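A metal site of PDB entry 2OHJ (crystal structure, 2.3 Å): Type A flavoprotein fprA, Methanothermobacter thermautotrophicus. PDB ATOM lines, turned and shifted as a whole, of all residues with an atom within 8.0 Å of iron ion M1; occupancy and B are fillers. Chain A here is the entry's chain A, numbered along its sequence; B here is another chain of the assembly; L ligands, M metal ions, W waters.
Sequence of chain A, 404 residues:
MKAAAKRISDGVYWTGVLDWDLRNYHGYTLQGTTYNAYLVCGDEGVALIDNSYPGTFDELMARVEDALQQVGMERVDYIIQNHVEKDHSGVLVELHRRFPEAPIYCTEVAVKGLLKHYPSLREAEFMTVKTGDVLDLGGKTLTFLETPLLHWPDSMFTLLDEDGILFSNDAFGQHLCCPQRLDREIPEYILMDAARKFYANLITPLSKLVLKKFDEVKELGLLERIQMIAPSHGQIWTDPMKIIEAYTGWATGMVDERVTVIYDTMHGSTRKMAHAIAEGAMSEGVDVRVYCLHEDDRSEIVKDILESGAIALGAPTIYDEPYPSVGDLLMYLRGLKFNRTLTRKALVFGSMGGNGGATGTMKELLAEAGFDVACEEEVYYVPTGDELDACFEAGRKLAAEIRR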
ATOM      1  N   TYR A  25      30.817   2.476  11.097  1.00  0.00           N
ATOM      2  CA  TYR A  25      30.703   3.418  12.217  1.00  0.00           C
ATOM      3  C   TYR A  25      31.173   2.795  13.537  1.00  0.00           C
ATOM      4  O   TYR A  25      31.187   1.576  13.678  1.00  0.00           O
ATOM      5  CB  TYR A  25      29.283   4.055  12.266  1.00  0.00           C
ATOM      6  CG  TYR A  25      28.232   3.347  13.083  1.00  0.00           C
ATOM      7  CD1 TYR A  25      27.286   4.084  13.799  1.00  0.00           C
ATOM      8  CD2 TYR A  25      28.155   1.950  13.145  1.00  0.00           C
ATOM      9  CE1 TYR A  25      26.305   3.470  14.558  1.00  0.00           C
ATOM     10  CE2 TYR A  25      27.177   1.303  13.906  1.00  0.00           C
ATOM     11  CZ  TYR A  25      26.250   2.079  14.612  1.00  0.00           C
ATOM     12  OH  TYR A  25      25.260   1.465  15.382  1.00  0.00           O
ATOM     13  N   HIS A  26      31.590   3.633  14.491  1.00  0.00           N
ATOM     14  CA  HIS A  26      32.140   3.140  15.763  1.00  0.00           C
ATOM     15  C   HIS A  26      33.402   2.261  15.618  1.00  0.00           C
ATOM     16  O   HIS A  26      33.661   1.412  16.482  1.00  0.00           O
ATOM     17  CB  HIS A  26      31.101   2.321  16.549  1.00  0.00           C
ATOM     18  CG  HIS A  26      29.876   3.072  16.929  1.00  0.00           C
ATOM     19  ND1 HIS A  26      28.669   2.446  17.168  1.00  0.00           N
ATOM     20  CD2 HIS A  26      29.644   4.397  17.118  1.00  0.00           C
ATOM     21  CE1 HIS A  26      27.765   3.343  17.492  1.00  0.00           C
ATOM     22  NE2 HIS A  26      28.331   4.539  17.465  1.00  0.00           N
ATOM     23  N   TYR A  35      17.720  -0.107  14.514  1.00  0.00           N
ATOM     24  CA  TYR A  35      17.556   0.437  15.847  1.00  0.00           C
ATOM     25  C   TYR A  35      16.215  -0.056  16.352  1.00  0.00           C
ATOM     26  O   TYR A  35      15.163   0.446  15.956  1.00  0.00           O
ATOM     27  CB  TYR A  35      17.645   1.961  15.820  1.00  0.00           C
ATOM     28  CG  TYR A  35      18.783   2.404  14.950  1.00  0.00           C
ATOM     29  CD1 TYR A  35      20.094   2.092  15.303  1.00  0.00           C
ATOM     30  CD2 TYR A  35      18.565   3.053  13.761  1.00  0.00           C
ATOM     31  CE1 TYR A  35      21.167   2.459  14.496  1.00  0.00           C
ATOM     32  CE2 TYR A  35      19.631   3.435  12.947  1.00  0.00           C
ATOM     33  CZ  TYR A  35      20.923   3.123  13.321  1.00  0.00           C
ATOM     34  OH  TYR A  35      21.986   3.490  12.524  1.00  0.00           O
ATOM     35  N   TYR A  53      18.206   6.546  15.917  1.00  0.00           N
ATOM     36  CA  TYR A  53      19.140   7.569  15.425  1.00  0.00           C
ATOM     37  C   TYR A  53      18.434   8.890  15.067  1.00  0.00           C
ATOM     38  O   TYR A  53      17.277   8.881  14.645  1.00  0.00           O
ATOM     39  CB  TYR A  53      19.928   7.009  14.219  1.00  0.00           C
ATOM     40  CG  TYR A  53      21.149   7.815  13.854  1.00  0.00           C
ATOM     41  CD1 TYR A  53      22.370   7.599  14.493  1.00  0.00           C
ATOM     42  CD2 TYR A  53      21.088   8.801  12.850  1.00  0.00           C
ATOM     43  CE1 TYR A  53      23.502   8.322  14.167  1.00  0.00           C
ATOM     44  CE2 TYR A  53      22.239   9.565  12.514  1.00  0.00           C
ATOM     45  CZ  TYR A  53      23.441   9.305  13.172  1.00  0.00           C
ATOM     46  OH  TYR A  53      24.585  10.024  12.887  1.00  0.00           O
ATOM     47  N   VAL A  84      22.031   5.831  26.589  1.00  0.00           N
ATOM     48  CA  VAL A  84      22.037   7.206  26.054  1.00  0.00           C
ATOM     49  C   VAL A  84      22.550   7.327  24.612  1.00  0.00           C
ATOM     50  O   VAL A  84      22.242   8.301  23.928  1.00  0.00           O
ATOM     51  CB  VAL A  84      22.781   8.209  26.990  1.00  0.00           C
ATOM     52  CG1 VAL A  84      22.275   8.081  28.410  1.00  0.00           C
ATOM     53  CG2 VAL A  84      24.296   8.051  26.938  1.00  0.00           C
ATOM     54  N   GLU A  85      23.357   6.358  24.175  1.00  0.00           N
ATOM     55  CA  GLU A  85      23.933   6.330  22.826  1.00  0.00           C
ATOM     56  C   GLU A  85      22.955   6.864  21.775  1.00  0.00           C
ATOM     57  O   GLU A  85      21.781   6.488  21.772  1.00  0.00           O
ATOM     58  CB  GLU A  85      24.422   4.905  22.525  1.00  0.00           C
ATOM     59  CG  GLU A  85      24.372   4.447  21.082  1.00  0.00           C
ATOM     60  CD  GLU A  85      25.484   5.028  20.240  1.00  0.00           C
ATOM     61  OE1 GLU A  85      25.184   5.490  19.114  1.00  0.00           O
ATOM     62  OE2 GLU A  85      26.650   5.027  20.690  1.00  0.00           O
ATOM     63  N   LYS A  86      23.434   7.742  20.884  1.00  0.00           N
ATOM     64  CA  LYS A  86      22.508   8.484  19.994  1.00  0.00           C
ATOM     65  C   LYS A  86      21.746   7.596  19.007  1.00  0.00           C
ATOM     66  O   LYS A  86      20.638   7.956  18.594  1.00  0.00           O
ATOM     67  CB  LYS A  86      23.179   9.677  19.292  1.00  0.00           C
ATOM     68  CG  LYS A  86      24.118   9.338  18.146  1.00  0.00           C
ATOM     69  CD  LYS A  86      24.978  10.538  17.745  1.00  0.00           C
ATOM     70  CE  LYS A  86      24.284  11.460  16.758  1.00  0.00           C
ATOM     71  NZ  LYS A  86      25.295  12.271  16.032  1.00  0.00           N
ATOM     72  N   ASP A  87      22.340   6.448  18.646  1.00  0.00           N
ATOM     73  CA  ASP A  87      21.622   5.348  17.964  1.00  0.00           C
ATOM     74  C   ASP A  87      20.262   5.035  18.611  1.00  0.00           C
ATOM     75  O   ASP A  87      19.348   4.573  17.929  1.00  0.00           O
ATOM     76  CB  ASP A  87      22.440   4.064  18.042  1.00  0.00           C
ATOM     77  CG  ASP A  87      23.560   3.998  17.053  1.00  0.00           C
ATOM     78  OD1 ASP A  87      24.194   2.923  17.013  1.00  0.00           O
ATOM     79  OD2 ASP A  87      23.819   4.985  16.327  1.00  0.00           O
ATOM     80  N   HIS A  88      20.158   5.280  19.924  1.00  0.00           N
ATOM     81  CA  HIS A  88      19.049   4.762  20.731  1.00  0.00           C
ATOM     82  C   HIS A  88      18.257   5.832  21.445  1.00  0.00           C
ATOM     83  O   HIS A  88      17.163   5.560  21.926  1.00  0.00           O
ATOM     84  CB  HIS A  88      19.566   3.740  21.744  1.00  0.00           C
ATOM     85  CG  HIS A  88      20.347   2.640  21.105  1.00  0.00           C
ATOM     86  ND1 HIS A  88      19.788   1.746  20.219  1.00  0.00           N
ATOM     87  CD2 HIS A  88      21.657   2.315  21.195  1.00  0.00           C
ATOM     88  CE1 HIS A  88      20.721   0.911  19.797  1.00  0.00           C
ATOM     89  NE2 HIS A  88      21.859   1.227  20.366  1.00  0.00           N
ATOM     90  N   HIS A 117      23.711  15.555  25.947  1.00  0.00           N
ATOM     91  CA  HIS A 117      23.327  15.452  24.541  1.00  0.00           C
ATOM     92  C   HIS A 117      22.162  16.407  24.198  1.00  0.00           C
ATOM     93  O   HIS A 117      22.176  17.073  23.158  1.00  0.00           O
ATOM     94  CB  HIS A 117      22.894  14.027  24.183  1.00  0.00           C
ATOM     95  CG  HIS A 117      24.020  13.059  24.024  1.00  0.00           C
ATOM     96  ND1 HIS A 117      24.542  12.345  25.079  1.00  0.00           N
ATOM     97  CD2 HIS A 117      24.688  12.651  22.923  1.00  0.00           C
ATOM     98  CE1 HIS A 117      25.492  11.544  24.636  1.00  0.00           C
ATOM     99  NE2 HIS A 117      25.603  11.711  23.333  1.00  0.00           N
ATOM    100  N   ASP A 170      22.230  -3.112  24.065  1.00  0.00           N
ATOM    101  CA  ASP A 170      23.175  -3.641  23.064  1.00  0.00           C
ATOM    102  C   ASP A 170      23.733  -5.042  23.349  1.00  0.00           C
ATOM    103  O   ASP A 170      24.282  -5.699  22.450  1.00  0.00           O
ATOM    104  CB  ASP A 170      24.280  -2.608  22.761  1.00  0.00           C
ATOM    105  CG  ASP A 170      23.865  -1.580  21.708  1.00  0.00           C
ATOM    106  OD1 ASP A 170      22.658  -1.417  21.449  1.00  0.00           O
ATOM    107  OD2 ASP A 170      24.711  -0.925  21.085  1.00  0.00           O
ATOM    108  N   HIS A 233      19.931  -3.899  18.437  1.00  0.00           N
ATOM    109  CA  HIS A 233      20.326  -4.027  17.041  1.00  0.00           C
ATOM    110  C   HIS A 233      20.091  -5.464  16.615  1.00  0.00           C
ATOM    111  O   HIS A 233      20.403  -6.399  17.352  1.00  0.00           O
ATOM    112  CB  HIS A 233      21.814  -3.742  16.841  1.00  0.00           C
ATOM    113  CG  HIS A 233      22.267  -2.386  17.274  1.00  0.00           C
ATOM    114  ND1 HIS A 233      22.132  -1.258  16.486  1.00  0.00           N
ATOM    115  CD2 HIS A 233      22.921  -1.978  18.399  1.00  0.00           C
ATOM    116  CE1 HIS A 233      22.646  -0.219  17.121  1.00  0.00           C
ATOM    117  NE2 HIS A 233      23.135  -0.632  18.281  1.00  0.00           N
ATOM    118  N   MET B 266      33.342  10.148  16.046  1.00  0.00           N
ATOM    119  CA  MET B 266      32.272   9.187  15.736  1.00  0.00           C
ATOM    120  C   MET B 266      30.926   9.881  15.623  1.00  0.00           C
ATOM    121  O   MET B 266      30.195   9.664  14.654  1.00  0.00           O
ATOM    122  CB  MET B 266      32.219   8.061  16.774  1.00  0.00           C
ATOM    123  CG  MET B 266      33.416   7.102  16.711  1.00  0.00           C
ATOM    124  SD  MET B 266      33.376   5.830  18.000  1.00  0.00           S
ATOM    125  CE  MET B 266      33.570   6.874  19.469  1.00  0.00           C
ATOM    126  N   HIS B 267      30.613  10.722  16.603  1.00  0.00           N
ATOM    127  CA  HIS B 267      29.317  11.382  16.719  1.00  0.00           C
ATOM    128  C   HIS B 267      29.406  12.892  16.470  1.00  0.00           C
ATOM    129  O   HIS B 267      28.414  13.600  16.629  1.00  0.00           O
ATOM    130  CB  HIS B 267      28.730  11.142  18.119  1.00  0.00           C
ATOM    131  CG  HIS B 267      28.415   9.709  18.421  1.00  0.00           C
ATOM    132  ND1 HIS B 267      28.347   9.215  19.706  1.00  0.00           N
ATOM    133  CD2 HIS B 267      28.142   8.657  17.604  1.00  0.00           C
ATOM    134  CE1 HIS B 267      28.045   7.933  19.677  1.00  0.00           C
ATOM    135  NE2 HIS B 267      27.916   7.564  18.414  1.00  0.00           N
HETATM  136  N1  LIG L   1      34.041   6.855  26.628  1.00  0.00           N
HETATM  137  C1  LIG L   1      34.894   6.731  27.709  1.00  0.00           C
HETATM  138  O1  LIG L   1      35.074   7.672  28.475  1.00  0.00           O
HETATM  139  N2  LIG L   1      35.565   5.566  27.924  1.00  0.00           N
HETATM  140  C2  LIG L   1      35.390   4.493  27.091  1.00  0.00           C
HETATM  141  O2  LIG L   1      35.955   3.425  27.364  1.00  0.00           O
HETATM  142  C3  LIG L   1      34.522   4.600  26.005  1.00  0.00           C
HETATM  143  N3  LIG L   1      34.325   3.528  25.151  1.00  0.00           N
HETATM  144  C4  LIG L   1      33.494   3.616  24.059  1.00  0.00           C
HETATM  145  C5  LIG L   1      33.359   2.498  23.234  1.00  0.00           C
HETATM  146  C6  LIG L   1      32.526   2.540  22.120  1.00  0.00           C
HETATM  147  C7  LIG L   1      32.698   1.478  21.069  1.00  0.00           C
HETATM  148  C8  LIG L   1      31.822   3.724  21.827  1.00  0.00           C
HETATM  149  C9  LIG L   1      30.995   3.837  20.566  1.00  0.00           C
HETATM  150  C10 LIG L   1      31.959   4.847  22.674  1.00  0.00           C
HETATM  151  C11 LIG L   1      32.805   4.809  23.800  1.00  0.00           C
HETATM  152  N4  LIG L   1      32.985   5.895  24.658  1.00  0.00           N
HETATM  153  C12 LIG L   1      33.843   5.788  25.754  1.00  0.00           C
HETATM  154  C13 LIG L   1      32.103   7.132  24.578  1.00  0.00           C
HETATM  155  C14 LIG L   1      32.613   8.174  23.566  1.00  0.00           C
HETATM  156  O3  LIG L   1      33.946   8.577  23.825  1.00  0.00           O
HETATM  157  C15 LIG L   1      31.673   9.396  23.596  1.00  0.00           C
HETATM  158  O4  LIG L   1      30.466   9.072  22.964  1.00  0.00           O
HETATM  159  C16 LIG L   1      32.272  10.655  22.954  1.00  0.00           C
HETATM  160  O5  LIG L   1      31.448  11.749  23.301  1.00  0.00           O
HETATM  161  C17 LIG L   1      32.431  10.524  21.444  1.00  0.00           C
HETATM  162  O6  LIG L   1      32.965  11.706  20.874  1.00  0.00           O
HETATM  163  P1  LIG L   1      32.776  12.035  19.306  1.00  0.00           P
HETATM  164  O7  LIG L   1      31.547  12.875  19.171  1.00  0.00           O
HETATM  165  O8  LIG L   1      33.907  12.896  18.790  1.00  0.00           O
HETATM  166  O9  LIG L   1      32.761  10.754  18.529  1.00  0.00           O
HETATM  167 FE    FE M   1      26.998   5.960  18.082  1.00  0.00          FE
HETATM  168 FE    FE M   2      23.644   0.293  20.078  1.00  0.00          FE
HETATM  169  O   HOH W   1      25.959   6.446  16.634  1.00  0.00           O
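The backbone NH of His 267 of chain B is in hydrogen-bond range of an oxygen (O9) of the ligand, 2.9 Å away. N of Met 266 of chain B lies within hydrogen-bond range of O9 of the ligand (2.6 Å).
O of His 267 of chain B is in hydrogen-bond range of NZ of Lys 86, 3.4 Å away. The side-chain carboxylate (OE1) of Glu 85 lies close to the backbone NH (N) of Asp 87 (3.0 Å). OH of Tyr 25 sits at hydrogen-bond distance from OD1 of Asp 87, 2.4 Å away. The backbone NH (N) of Tyr 53 lies within hydrogen-bond range of the backbone carbonyl oxygen (O) of Asp 87 (3.0 Å).
OD2 of Asp 87 touches iron ion M1, 3.8 Å away. Within 4 Å of iron ion M1: His 26, Glu 85, Asp 87 and His 267 of chain B. The nearest printed residue that does not touch iron ion M1 is Tyr 25 (4.4 Å).
Water W1 binds iron ion M1, at 1.8 Å. Iron ion M1 is bound by NE2 of His 267 of chain B (1.9 Å). NE2 of His 26 is bound to iron ion M1 (2.0 Å). Iron ion M1 is bound by OE1 of Glu 85, at 2.1 Å. Slightly farther from iron ion M1 lies the side-chain carboxylate (OE2) of Glu 85 (2.8 Å).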
